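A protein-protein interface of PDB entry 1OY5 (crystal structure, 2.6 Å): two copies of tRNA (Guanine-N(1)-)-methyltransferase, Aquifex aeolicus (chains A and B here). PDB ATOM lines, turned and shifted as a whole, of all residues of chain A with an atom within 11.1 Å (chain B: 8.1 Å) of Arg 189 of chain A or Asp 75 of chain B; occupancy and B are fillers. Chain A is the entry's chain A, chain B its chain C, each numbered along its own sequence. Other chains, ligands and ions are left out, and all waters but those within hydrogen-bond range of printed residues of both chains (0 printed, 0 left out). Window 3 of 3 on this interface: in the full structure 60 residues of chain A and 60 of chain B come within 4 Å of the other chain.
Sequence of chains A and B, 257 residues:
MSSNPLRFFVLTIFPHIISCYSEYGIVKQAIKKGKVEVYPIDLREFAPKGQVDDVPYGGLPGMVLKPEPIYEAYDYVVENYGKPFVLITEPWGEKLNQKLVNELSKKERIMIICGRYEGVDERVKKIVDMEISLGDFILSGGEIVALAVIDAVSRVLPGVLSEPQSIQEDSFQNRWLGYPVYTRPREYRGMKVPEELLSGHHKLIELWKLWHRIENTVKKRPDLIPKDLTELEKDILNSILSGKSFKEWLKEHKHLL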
ATOM      1  N   THR A 183     -23.006 -16.339   5.115  1.00  0.00           N
ATOM      2  CA  THR A 183     -23.957 -16.917   6.058  1.00  0.00           C
ATOM      3  C   THR A 183     -25.387 -16.316   6.031  1.00  0.00           C
ATOM      4  O   THR A 183     -25.638 -15.236   5.473  1.00  0.00           O
ATOM      5  CB  THR A 183     -23.417 -16.916   7.462  1.00  0.00           C
ATOM      6  OG1 THR A 183     -24.286 -17.730   8.249  1.00  0.00           O
ATOM      7  CG2 THR A 183     -23.483 -15.506   8.097  1.00  0.00           C
ATOM      8  N   ARG A 184     -26.277 -17.013   6.736  1.00  0.00           N
ATOM      9  CA  ARG A 184     -27.749 -16.885   6.626  1.00  0.00           C
ATOM     10  C   ARG A 184     -28.485 -15.609   6.205  1.00  0.00           C
ATOM     11  O   ARG A 184     -29.504 -15.732   5.514  1.00  0.00           O
ATOM     12  CB  ARG A 184     -28.468 -17.625   7.748  1.00  0.00           C
ATOM     13  CG  ARG A 184     -29.516 -18.592   7.143  1.00  0.00           C
ATOM     14  CD  ARG A 184     -29.017 -20.027   6.871  1.00  0.00           C
ATOM     15  NE  ARG A 184     -28.454 -20.262   5.542  1.00  0.00           N
ATOM     16  CZ  ARG A 184     -28.182 -21.476   5.068  1.00  0.00           C
ATOM     17  NH1 ARG A 184     -28.419 -22.550   5.804  1.00  0.00           N
ATOM     18  NH2 ARG A 184     -27.669 -21.632   3.860  1.00  0.00           N
ATOM     19  N   PRO A 185     -28.184 -14.420   6.692  1.00  0.00           N
ATOM     20  CA  PRO A 185     -28.669 -13.245   5.971  1.00  0.00           C
ATOM     21  C   PRO A 185     -28.425 -13.305   4.456  1.00  0.00           C
ATOM     22  O   PRO A 185     -27.368 -12.930   3.973  1.00  0.00           O
ATOM     23  CB  PRO A 185     -27.922 -12.106   6.651  1.00  0.00           C
ATOM     24  CG  PRO A 185     -27.845 -12.553   8.065  1.00  0.00           C
ATOM     25  CD  PRO A 185     -27.756 -14.069   8.055  1.00  0.00           C
ATOM     26  N   ARG A 186     -29.435 -13.760   3.718  1.00  0.00           N
ATOM     27  CA  ARG A 186     -29.346 -13.919   2.257  1.00  0.00           C
ATOM     28  C   ARG A 186     -29.052 -12.600   1.550  1.00  0.00           C
ATOM     29  O   ARG A 186     -28.255 -12.543   0.619  1.00  0.00           O
ATOM     30  CB  ARG A 186     -30.637 -14.514   1.704  1.00  0.00           C
ATOM     31  CG  ARG A 186     -30.629 -14.691   0.191  1.00  0.00           C
ATOM     32  CD  ARG A 186     -32.006 -14.949  -0.378  1.00  0.00           C
ATOM     33  NE  ARG A 186     -32.061 -14.997  -1.840  1.00  0.00           N
ATOM     34  CZ  ARG A 186     -31.803 -13.970  -2.654  1.00  0.00           C
ATOM     35  NH1 ARG A 186     -31.438 -12.780  -2.171  1.00  0.00           N
ATOM     36  NH2 ARG A 186     -31.909 -14.143  -3.972  1.00  0.00           N
ATOM     37  N   GLU A 187     -29.731 -11.547   1.970  1.00  0.00           N
ATOM     38  CA  GLU A 187     -29.432 -10.223   1.457  1.00  0.00           C
ATOM     39  C   GLU A 187     -29.334  -9.257   2.629  1.00  0.00           C
ATOM     40  O   GLU A 187     -30.188  -9.253   3.512  1.00  0.00           O
ATOM     41  CB  GLU A 187     -30.498  -9.774   0.472  1.00  0.00           C
ATOM     42  CG  GLU A 187     -30.298  -8.370  -0.068  1.00  0.00           C
ATOM     43  CD  GLU A 187     -31.252  -8.076  -1.203  1.00  0.00           C
ATOM     44  OE1 GLU A 187     -31.246  -6.938  -1.732  1.00  0.00           O
ATOM     45  OE2 GLU A 187     -32.011  -9.001  -1.574  1.00  0.00           O
ATOM     46  N   TYR A 188     -28.287  -8.447   2.647  1.00  0.00           N
ATOM     47  CA  TYR A 188     -28.104  -7.484   3.728  1.00  0.00           C
ATOM     48  C   TYR A 188     -27.547  -6.167   3.194  1.00  0.00           C
ATOM     49  O   TYR A 188     -26.633  -6.161   2.382  1.00  0.00           O
ATOM     50  CB  TYR A 188     -27.187  -8.072   4.791  1.00  0.00           C
ATOM     51  CG  TYR A 188     -26.966  -7.174   5.979  1.00  0.00           C
ATOM     52  CD1 TYR A 188     -25.748  -6.563   6.183  1.00  0.00           C
ATOM     53  CD2 TYR A 188     -27.969  -6.948   6.905  1.00  0.00           C
ATOM     54  CE1 TYR A 188     -25.534  -5.745   7.277  1.00  0.00           C
ATOM     55  CE2 TYR A 188     -27.763  -6.134   7.993  1.00  0.00           C
ATOM     56  CZ  TYR A 188     -26.542  -5.537   8.176  1.00  0.00           C
ATOM     57  OH  TYR A 188     -26.317  -4.732   9.264  1.00  0.00           O
ATOM     58  N   ARG A 189     -28.121  -5.053   3.634  1.00  0.00           N
ATOM     59  CA  ARG A 189     -27.672  -3.742   3.182  1.00  0.00           C
ATOM     60  C   ARG A 189     -27.537  -3.741   1.670  1.00  0.00           C
ATOM     61  O   ARG A 189     -26.601  -3.149   1.150  1.00  0.00           O
ATOM     62  CB  ARG A 189     -26.303  -3.387   3.776  1.00  0.00           C
ATOM     63  CG  ARG A 189     -26.226  -3.349   5.302  1.00  0.00           C
ATOM     64  CD  ARG A 189     -26.980  -2.203   5.882  1.00  0.00           C
ATOM     65  NE  ARG A 189     -26.799  -1.969   7.314  1.00  0.00           N
ATOM     66  CZ  ARG A 189     -25.712  -1.432   7.886  1.00  0.00           C
ATOM     67  NH1 ARG A 189     -24.645  -1.127   7.165  1.00  0.00           N
ATOM     68  NH2 ARG A 189     -25.692  -1.206   9.196  1.00  0.00           N
ATOM     69  N   GLY A 190     -28.433  -4.429   0.965  1.00  0.00           N
ATOM     70  CA  GLY A 190     -28.363  -4.509  -0.484  1.00  0.00           C
ATOM     71  C   GLY A 190     -27.313  -5.489  -0.990  1.00  0.00           C
ATOM     72  O   GLY A 190     -27.252  -5.779  -2.175  1.00  0.00           O
ATOM     73  N   MET A 191     -26.464  -5.990  -0.103  1.00  0.00           N
ATOM     74  CA  MET A 191     -25.459  -6.964  -0.500  1.00  0.00           C
ATOM     75  C   MET A 191     -26.100  -8.354  -0.507  1.00  0.00           C
ATOM     76  O   MET A 191     -26.665  -8.787   0.503  1.00  0.00           O
ATOM     77  CB  MET A 191     -24.241  -6.895   0.432  1.00  0.00           C
ATOM     78  CG  MET A 191     -23.419  -5.623   0.207  1.00  0.00           C
ATOM     79  SD  MET A 191     -22.078  -5.340   1.342  1.00  0.00           S
ATOM     80  CE  MET A 191     -22.948  -4.758   2.733  1.00  0.00           C
ATOM     81  N   LYS A 192     -26.036  -9.042  -1.644  1.00  0.00           N
ATOM     82  CA  LYS A 192     -26.629 -10.370  -1.739  1.00  0.00           C
ATOM     83  C   LYS A 192     -25.585 -11.470  -1.845  1.00  0.00           C
ATOM     84  O   LYS A 192     -24.490 -11.247  -2.357  1.00  0.00           O
ATOM     85  CB  LYS A 192     -27.577 -10.461  -2.929  1.00  0.00           C
ATOM     86  CG  LYS A 192     -28.726  -9.489  -2.825  1.00  0.00           C
ATOM     87  CD  LYS A 192     -29.820  -9.731  -3.861  1.00  0.00           C
ATOM     88  CE  LYS A 192     -29.376  -9.378  -5.260  1.00  0.00           C
ATOM     89  NZ  LYS A 192     -30.478  -9.599  -6.233  1.00  0.00           N
ATOM     90  N   VAL A 193     -25.934 -12.652  -1.341  1.00  0.00           N
ATOM     91  CA  VAL A 193     -25.068 -13.815  -1.438  1.00  0.00           C
ATOM     92  C   VAL A 193     -25.081 -14.312  -2.866  1.00  0.00           C
ATOM     93  O   VAL A 193     -26.139 -14.406  -3.467  1.00  0.00           O
ATOM     94  CB  VAL A 193     -25.583 -14.998  -0.590  1.00  0.00           C
ATOM     95  CG1 VAL A 193     -24.742 -16.247  -0.858  1.00  0.00           C
ATOM     96  CG2 VAL A 193     -25.583 -14.660   0.897  1.00  0.00           C
ATOM     97  N   PHE B  46     -24.395  -6.666  20.040  1.00  0.00           N
ATOM     98  CA  PHE B  46     -24.917  -6.143  18.789  1.00  0.00           C
ATOM     99  C   PHE B  46     -25.658  -7.217  18.071  1.00  0.00           C
ATOM    100  O   PHE B  46     -25.884  -7.156  16.887  1.00  0.00           O
ATOM    101  CB  PHE B  46     -23.792  -5.577  17.942  1.00  0.00           C
ATOM    102  CG  PHE B  46     -23.216  -4.352  18.525  1.00  0.00           C
ATOM    103  CD1 PHE B  46     -23.775  -3.123  18.261  1.00  0.00           C
ATOM    104  CD2 PHE B  46     -22.165  -4.427  19.413  1.00  0.00           C
ATOM    105  CE1 PHE B  46     -23.249  -1.982  18.837  1.00  0.00           C
ATOM    106  CE2 PHE B  46     -21.649  -3.299  19.982  1.00  0.00           C
ATOM    107  CZ  PHE B  46     -22.191  -2.068  19.685  1.00  0.00           C
ATOM    108  N   PRO B  67     -23.002 -11.058   9.109  1.00  0.00           N
ATOM    109  CA  PRO B  67     -22.752  -9.674   8.710  1.00  0.00           C
ATOM    110  C   PRO B  67     -23.327  -8.616   9.654  1.00  0.00           C
ATOM    111  O   PRO B  67     -22.619  -7.662  10.009  1.00  0.00           O
ATOM    112  CB  PRO B  67     -23.461  -9.583   7.363  1.00  0.00           C
ATOM    113  CG  PRO B  67     -23.579 -10.963   6.918  1.00  0.00           C
ATOM    114  CD  PRO B  67     -23.848 -11.761   8.135  1.00  0.00           C
ATOM    115  N   GLU B  68     -24.577  -8.783  10.074  1.00  0.00           N
ATOM    116  CA  GLU B  68     -25.271  -7.737  10.865  1.00  0.00           C
ATOM    117  C   GLU B  68     -24.547  -7.207  12.122  1.00  0.00           C
ATOM    118  O   GLU B  68     -24.313  -6.015  12.211  1.00  0.00           O
ATOM    119  CB  GLU B  68     -26.689  -8.177  11.242  1.00  0.00           C
ATOM    120  CG  GLU B  68     -27.472  -8.787  10.095  1.00  0.00           C
ATOM    121  CD  GLU B  68     -27.468 -10.305  10.137  1.00  0.00           C
ATOM    122  OE1 GLU B  68     -28.552 -10.884  10.376  1.00  0.00           O
ATOM    123  OE2 GLU B  68     -26.395 -10.926   9.946  1.00  0.00           O
ATOM    124  N   PRO B  69     -24.196  -8.067  13.085  1.00  0.00           N
ATOM    125  CA  PRO B  69     -23.571  -7.588  14.321  1.00  0.00           C
ATOM    126  C   PRO B  69     -22.247  -6.888  14.083  1.00  0.00           C
ATOM    127  O   PRO B  69     -21.991  -5.845  14.717  1.00  0.00           O
ATOM    128  CB  PRO B  69     -23.409  -8.862  15.148  1.00  0.00           C
ATOM    129  CG  PRO B  69     -24.441  -9.743  14.607  1.00  0.00           C
ATOM    130  CD  PRO B  69     -24.367  -9.528  13.115  1.00  0.00           C
ATOM    131  N   ILE B  70     -21.454  -7.416  13.152  1.00  0.00           N
ATOM    132  CA  ILE B  70     -20.182  -6.770  12.811  1.00  0.00           C
ATOM    133  C   ILE B  70     -20.425  -5.406  12.184  1.00  0.00           C
ATOM    134  O   ILE B  70     -19.707  -4.477  12.490  1.00  0.00           O
ATOM    135  CB  ILE B  70     -19.294  -7.646  11.873  1.00  0.00           C
ATOM    136  CG1 ILE B  70     -18.913  -8.960  12.564  1.00  0.00           C
ATOM    137  CG2 ILE B  70     -18.016  -6.874  11.483  1.00  0.00           C
ATOM    138  CD1 ILE B  70     -18.189  -9.942  11.648  1.00  0.00           C
ATOM    139  N   TYR B  71     -21.415  -5.290  11.292  1.00  0.00           N
ATOM    140  CA  TYR B  71     -21.699  -3.998  10.653  1.00  0.00           C
ATOM    141  C   TYR B  71     -22.267  -3.027  11.685  1.00  0.00           C
ATOM    142  O   TYR B  71     -21.999  -1.830  11.659  1.00  0.00           O
ATOM    143  CB  TYR B  71     -22.684  -4.130   9.510  1.00  0.00           C
ATOM    144  CG  TYR B  71     -22.025  -4.190   8.162  1.00  0.00           C
ATOM    145  CD1 TYR B  71     -21.628  -3.023   7.502  1.00  0.00           C
ATOM    146  CD2 TYR B  71     -21.804  -5.425   7.530  1.00  0.00           C
ATOM    147  CE1 TYR B  71     -21.016  -3.095   6.259  1.00  0.00           C
ATOM    148  CE2 TYR B  71     -21.186  -5.508   6.301  1.00  0.00           C
ATOM    149  CZ  TYR B  71     -20.787  -4.360   5.668  1.00  0.00           C
ATOM    150  OH  TYR B  71     -20.176  -4.488   4.436  1.00  0.00           O
ATOM    151  N   GLU B  72     -23.061  -3.570  12.592  1.00  0.00           N
ATOM    152  CA  GLU B  72     -23.712  -2.757  13.592  1.00  0.00           C
ATOM    153  C   GLU B  72     -22.661  -2.177  14.531  1.00  0.00           C
ATOM    154  O   GLU B  72     -22.691  -0.993  14.860  1.00  0.00           O
ATOM    155  CB  GLU B  72     -24.683  -3.597  14.363  1.00  0.00           C
ATOM    156  CG  GLU B  72     -25.999  -2.954  14.567  1.00  0.00           C
ATOM    157  CD  GLU B  72     -26.689  -2.680  13.252  1.00  0.00           C
ATOM    158  OE1 GLU B  72     -26.718  -3.653  12.442  1.00  0.00           O
ATOM    159  OE2 GLU B  72     -27.208  -1.516  13.055  1.00  0.00           O
ATOM    160  N   ALA B  73     -21.745  -3.034  14.958  1.00  0.00           N
ATOM    161  CA  ALA B  73     -20.639  -2.637  15.823  1.00  0.00           C
ATOM    162  C   ALA B  73     -19.720  -1.659  15.055  1.00  0.00           C
ATOM    163  O   ALA B  73     -19.218  -0.726  15.621  1.00  0.00           O
ATOM    164  CB  ALA B  73     -19.864  -3.862  16.300  1.00  0.00           C
ATOM    165  N   TYR B  74     -19.515  -1.872  13.772  1.00  0.00           N
ATOM    166  CA  TYR B  74     -18.749  -0.919  12.986  1.00  0.00           C
ATOM    167  C   TYR B  74     -19.431   0.487  13.087  1.00  0.00           C
ATOM    168  O   TYR B  74     -18.805   1.474  13.509  1.00  0.00           O
ATOM    169  CB  TYR B  74     -18.627  -1.404  11.531  1.00  0.00           C
ATOM    170  CG  TYR B  74     -17.946  -0.442  10.605  1.00  0.00           C
ATOM    171  CD1 TYR B  74     -18.685   0.346   9.736  1.00  0.00           C
ATOM    172  CD2 TYR B  74     -16.564  -0.325  10.573  1.00  0.00           C
ATOM    173  CE1 TYR B  74     -18.066   1.247   8.853  1.00  0.00           C
ATOM    174  CE2 TYR B  74     -15.939   0.576   9.702  1.00  0.00           C
ATOM    175  CZ  TYR B  74     -16.698   1.343   8.847  1.00  0.00           C
ATOM    176  OH  TYR B  74     -16.101   2.229   7.994  1.00  0.00           O
ATOM    177  N   ASP B  75     -20.720   0.549  12.761  1.00  0.00           N
ATOM    178  CA  ASP B  75     -21.454   1.804  12.799  1.00  0.00           C
ATOM    179  C   ASP B  75     -21.321   2.463  14.148  1.00  0.00           C
ATOM    180  O   ASP B  75     -21.078   3.669  14.220  1.00  0.00           O
ATOM    181  CB  ASP B  75     -22.947   1.631  12.490  1.00  0.00           C
ATOM    182  CG  ASP B  75     -23.217   1.154  11.074  1.00  0.00           C
ATOM    183  OD1 ASP B  75     -24.375   0.763  10.848  1.00  0.00           O
ATOM    184  OD2 ASP B  75     -22.370   1.099  10.140  1.00  0.00           O
ATOM    185  N   TYR B  76     -21.513   1.684  15.210  1.00  0.00           N
ATOM    186  CA  TYR B  76     -21.430   2.182  16.576  1.00  0.00           C
ATOM    187  C   TYR B  76     -20.093   2.853  16.818  1.00  0.00           C
ATOM    188  O   TYR B  76     -20.029   3.875  17.464  1.00  0.00           O
ATOM    189  CB  TYR B  76     -21.627   1.054  17.590  1.00  0.00           C
ATOM    190  CG  TYR B  76     -21.296   1.457  19.029  1.00  0.00           C
ATOM    191  CD1 TYR B  76     -20.000   1.354  19.537  1.00  0.00           C
ATOM    192  CD2 TYR B  76     -22.275   1.914  19.866  1.00  0.00           C
ATOM    193  CE1 TYR B  76     -19.712   1.729  20.827  1.00  0.00           C
ATOM    194  CE2 TYR B  76     -21.999   2.306  21.130  1.00  0.00           C
ATOM    195  CZ  TYR B  76     -20.722   2.209  21.626  1.00  0.00           C
ATOM    196  OH  TYR B  76     -20.501   2.599  22.943  1.00  0.00           O
ATOM    197  N   VAL B  77     -19.031   2.298  16.263  1.00  0.00           N
ATOM    198  CA  VAL B  77     -17.704   2.855  16.459  1.00  0.00           C
ATOM    199  C   VAL B  77     -17.516   4.117  15.628  1.00  0.00           C
ATOM    200  O   VAL B  77     -17.029   5.115  16.142  1.00  0.00           O
ATOM    201  CB  VAL B  77     -16.612   1.796  16.162  1.00  0.00           C
ATOM    202  CG1 VAL B  77     -15.206   2.427  16.094  1.00  0.00           C
ATOM    203  CG2 VAL B  77     -16.678   0.686  17.216  1.00  0.00           C
ATOM    204  N   VAL B  78     -17.959   4.101  14.372  1.00  0.00           N
ATOM    205  CA  VAL B  78     -17.828   5.255  13.494  1.00  0.00           C
ATOM    206  C   VAL B  78     -18.596   6.426  14.069  1.00  0.00           C
ATOM    207  O   VAL B  78     -18.187   7.576  13.914  1.00  0.00           O
ATOM    208  CB  VAL B  78     -18.354   4.943  12.094  1.00  0.00           C
ATOM    209  CG1 VAL B  78     -18.597   6.222  11.265  1.00  0.00           C
ATOM    210  CG2 VAL B  78     -17.394   4.028  11.377  1.00  0.00           C
ATOM    211  N   GLU B  79     -19.712   6.131  14.736  1.00  0.00           N
ATOM    212  CA  GLU B  79     -20.567   7.158  15.320  1.00  0.00           C
ATOM    213  C   GLU B  79     -20.032   7.721  16.608  1.00  0.00           C
ATOM    214  O   GLU B  79     -20.007   8.930  16.802  1.00  0.00           O
ATOM    215  CB  GLU B  79     -21.929   6.588  15.647  1.00  0.00           C
ATOM    216  CG  GLU B  79     -22.749   6.145  14.462  1.00  0.00           C
ATOM    217  CD  GLU B  79     -24.187   5.882  14.877  1.00  0.00           C
ATOM    218  OE1 GLU B  79     -24.723   6.689  15.706  1.00  0.00           O
ATOM    219  OE2 GLU B  79     -24.758   4.857  14.396  1.00  0.00           O
ATOM    220  N   ASN B  80     -19.623   6.843  17.512  1.00  0.00           N
ATOM    221  CA  ASN B  80     -19.178   7.292  18.831  1.00  0.00           C
ATOM    222  C   ASN B  80     -17.741   7.747  18.882  1.00  0.00           C
ATOM    223  O   ASN B  80     -17.358   8.469  19.759  1.00  0.00           O
ATOM    224  CB  ASN B  80     -19.416   6.181  19.829  1.00  0.00           C
ATOM    225  CG  ASN B  80     -20.868   5.969  20.080  1.00  0.00           C
ATOM    226  OD1 ASN B  80     -21.398   6.452  21.058  1.00  0.00           O
ATOM    227  ND2 ASN B  80     -21.536   5.275  19.176  1.00  0.00           N
ATOM    228  N   TYR B  81     -16.948   7.283  17.933  1.00  0.00           N
ATOM    229  CA  TYR B  81     -15.552   7.640  17.821  1.00  0.00           C
ATOM    230  C   TYR B  81     -15.461   7.885  16.359  1.00  0.00           C
ATOM    231  O   TYR B  81     -16.467   7.783  15.681  1.00  0.00           O
ATOM    232  CB  TYR B  81     -14.694   6.457  18.237  1.00  0.00           C
ATOM    233  CG  TYR B  81     -15.111   5.886  19.561  1.00  0.00           C
ATOM    234  CD1 TYR B  81     -14.644   6.439  20.746  1.00  0.00           C
ATOM    235  CD2 TYR B  81     -16.012   4.842  19.638  1.00  0.00           C
ATOM    236  CE1 TYR B  81     -15.042   5.959  21.973  1.00  0.00           C
ATOM    237  CE2 TYR B  81     -16.414   4.335  20.873  1.00  0.00           C
ATOM    238  CZ  TYR B  81     -15.915   4.912  22.037  1.00  0.00           C
ATOM    239  OH  TYR B  81     -16.287   4.456  23.281  1.00  0.00           O
ATOM    240  N   GLY B  82     -14.294   8.186  15.834  1.00  0.00           N
ATOM    241  CA  GLY B  82     -14.194   8.428  14.398  1.00  0.00           C
ATOM    242  C   GLY B  82     -14.315   7.177  13.546  1.00  0.00           C
ATOM    243  O   GLY B  82     -14.520   6.071  14.087  1.00  0.00           O
ATOM    244  N   LYS B  83     -14.164   7.351  12.230  1.00  0.00           N
ATOM    245  CA  LYS B  83     -14.104   6.238  11.298  1.00  0.00           C
ATOM    246  C   LYS B  83     -12.813   5.502  11.594  1.00  0.00           C
ATOM    247  O   LYS B  83     -11.744   6.079  11.579  1.00  0.00           O
ATOM    248  CB  LYS B  83     -14.081   6.714   9.853  1.00  0.00           C
ATOM    249  CG  LYS B  83     -13.951   5.581   8.813  1.00  0.00           C
ATOM    250  CD  LYS B  83     -13.927   6.110   7.383  1.00  0.00           C
ATOM    251  CE  LYS B  83     -14.367   5.059   6.355  1.00  0.00           C
ATOM    252  NZ  LYS B  83     -13.260   4.405   5.603  1.00  0.00           N
ATOM    253  N   PRO B  84     -12.884   4.229  11.921  1.00  0.00           N
ATOM    254  CA  PRO B  84     -11.647   3.488  12.189  1.00  0.00           C
ATOM    255  C   PRO B  84     -11.028   2.833  10.977  1.00  0.00           C
ATOM    256  O   PRO B  84     -11.721   2.565   9.997  1.00  0.00           O
ATOM    257  CB  PRO B  84     -12.109   2.427  13.166  1.00  0.00           C
ATOM    258  CG  PRO B  84     -13.515   2.184  12.810  1.00  0.00           C
ATOM    259  CD  PRO B  84     -14.088   3.419  12.163  1.00  0.00           C
ATOM    260  N   MET B 111      -9.897  -0.615  14.342  1.00  0.00           N
ATOM    261  CA  MET B 111     -10.900  -1.595  14.634  1.00  0.00           C
ATOM    262  C   MET B 111     -10.319  -2.904  14.196  1.00  0.00           C
ATOM    263  O   MET B 111      -9.932  -3.029  13.031  1.00  0.00           O
ATOM    264  CB  MET B 111     -12.195  -1.313  13.877  1.00  0.00           C
ATOM    265  CG  MET B 111     -13.253  -2.340  14.208  1.00  0.00           C
ATOM    266  SD  MET B 111     -14.976  -1.951  13.833  1.00  0.00           S
ATOM    267  CE  MET B 111     -15.449  -1.460  15.193  1.00  0.00           C
ATOM    268  N   ARG B 123     -19.260 -10.300   2.895  1.00  0.00           N
ATOM    269  CA  ARG B 123     -19.882  -8.984   2.794  1.00  0.00           C
ATOM    270  C   ARG B 123     -19.268  -7.967   3.760  1.00  0.00           C
ATOM    271  O   ARG B 123     -19.349  -6.766   3.530  1.00  0.00           O
ATOM    272  CB  ARG B 123     -21.378  -9.110   3.022  1.00  0.00           C
ATOM    273  CG  ARG B 123     -22.053  -9.891   1.921  1.00  0.00           C
ATOM    274  CD  ARG B 123     -23.501 -10.232   2.185  1.00  0.00           C
ATOM    275  NE  ARG B 123     -23.628 -11.344   3.124  1.00  0.00           N
ATOM    276  CZ  ARG B 123     -24.783 -11.883   3.503  1.00  0.00           C
ATOM    277  NH1 ARG B 123     -25.922 -11.411   3.015  1.00  0.00           N
ATOM    278  NH2 ARG B 123     -24.803 -12.907   4.360  1.00  0.00           N
ATOM    279  N   ILE B 127     -15.886  -3.225   4.360  1.00  0.00           N
ATOM    280  CA  ILE B 127     -15.381  -2.254   5.320  1.00  0.00           C
ATOM    281  C   ILE B 127     -14.047  -2.712   5.934  1.00  0.00           C
ATOM    282  O   ILE B 127     -13.610  -2.172   6.926  1.00  0.00           O
ATOM    283  CB  ILE B 127     -16.407  -2.012   6.459  1.00  0.00           C
ATOM    284  CG1 ILE B 127     -16.611  -3.301   7.248  1.00  0.00           C
ATOM    285  CG2 ILE B 127     -17.721  -1.458   5.915  1.00  0.00           C
ATOM    286  CD1 ILE B 127     -17.549  -3.164   8.360  1.00  0.00           C
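OE2 of Glu 187 of chain A lies within salt-bridge range of NH1 of Arg 186 of chain A, at 3.9 Å. The backbone NH of Val 193 of chain A is in hydrogen-bond range of the backbone carbonyl oxygen of Arg 186 of chain A, 3.0 Å away. The guanidinium group of Arg 189 of chain A is in hydrogen-bond range of the side-chain hydroxyl of Tyr 188 of chain A (3.4 Å). The side-chain hydroxyl (OH) of Tyr 71 of chain B sits at hydrogen-bond distance from the backbone carbonyl oxygen (O) of Arg 123 of chain B (2.6 Å).
The guanidinium group of Arg 123 of chain B lies within hydrogen-bond range of the backbone carbonyl oxygen of Thr 183 of chain A. O of Pro 185 of chain A lies within hydrogen-bond range of NH2 of Arg 123 of chain B (2.6 Å). The side-chain hydroxyl (OH) of Tyr 188 of chain A sits at hydrogen-bond distance from the side-chain carboxylate (OE1) of Glu 72 of chain B (3.4 Å). NH2 of Arg 189 of chain A lies within salt-bridge range of OD1 of Asp 75 of chain B (2.9 Å). The side-chain hydroxyl of Tyr 71 of chain B sits close to the side-chain sulfur of Met 191 of chain A (3.7 Å). The side-chain sulfur (SD) of Met 191 of chain A lies close to the backbone carbonyl oxygen (O) of Arg 123 of chain B, at 3.8 Å.
Of the 11 printed residues of chain A, 8 touch a printed residue of chain B. Printed residues of chain A that touch a printed residue of chain B: Thr 183, Pro 185, Arg 186, Glu 187, Tyr 188, Arg 189, Met 191 and Val 193. Hydrophobic or aromatic side chains of chain A within 4 Å of the printed part of chain B: Pro 185, Tyr 188, Met 191 and Val 193. Along chain A the printed residues that touch a printed residue of chain B span positions 183 to 193. Among the printed residues, Asp or Glu carboxylates within 4 Å of a Lys or Arg side-chain nitrogen of the other chain: Arg 189 of chain A with Asp 75 of chain B (2.9 Å).
No position is printed for both chains.
Among the printed residues, pairs that only touch across the chains: Pro 185 of chain A with Glu 68 of chain B, Tyr 188 of chain A with Glu 68 of chain B, Arg 186 of chain A with Arg 123 of chain B, Arg 189 of chain A with Tyr 71 of chain B, Tyr 188 of chain A with Tyr 71 of chain B, Thr 183 of chain A with Pro 67 of chain B, Tyr 188 of chain A with Arg 123 of chain B, Val 193 of chain A with Arg 123 of chain B, Glu 187 of chain A with Arg 123 of chain B and Tyr 188 of chain A with Pro 67 of chain B.
Of the printed residues of chain B, Tyr 188 of chain A touches Pro 67, Glu 68, Tyr 71, Glu 72 and Arg 123. Arg 189 of chain A touches just these residues of chain B: Tyr 71 and Asp 75. Of the printed residues of chain B, Met 191 of chain A touches Tyr 71 (3.3 Å) and Arg 123 (3.7 Å). Of the printed residues of chain A, Pro 67 of chain B touches Thr 183 (3.8 Å) and Tyr 188 (3.97 Å). Of the printed residues of chain A, Glu 68 of chain B touches Pro 185 and Tyr 188. Tyr 71 of chain B touches three residues of chain A. No residue of chain A comes within 4 Å of Ala 73 of chain B. Tyr 74 of chain B touches none of the printed residues of chain A. Of chain A, only Arg 189 (2.9 Å) comes within 4 Å of Asp 75 of chain B. No residue of chain A comes within 4 Å of Val 77 of chain B. No residue of chain A comes within 4 Å of Glu 79 of chain B.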
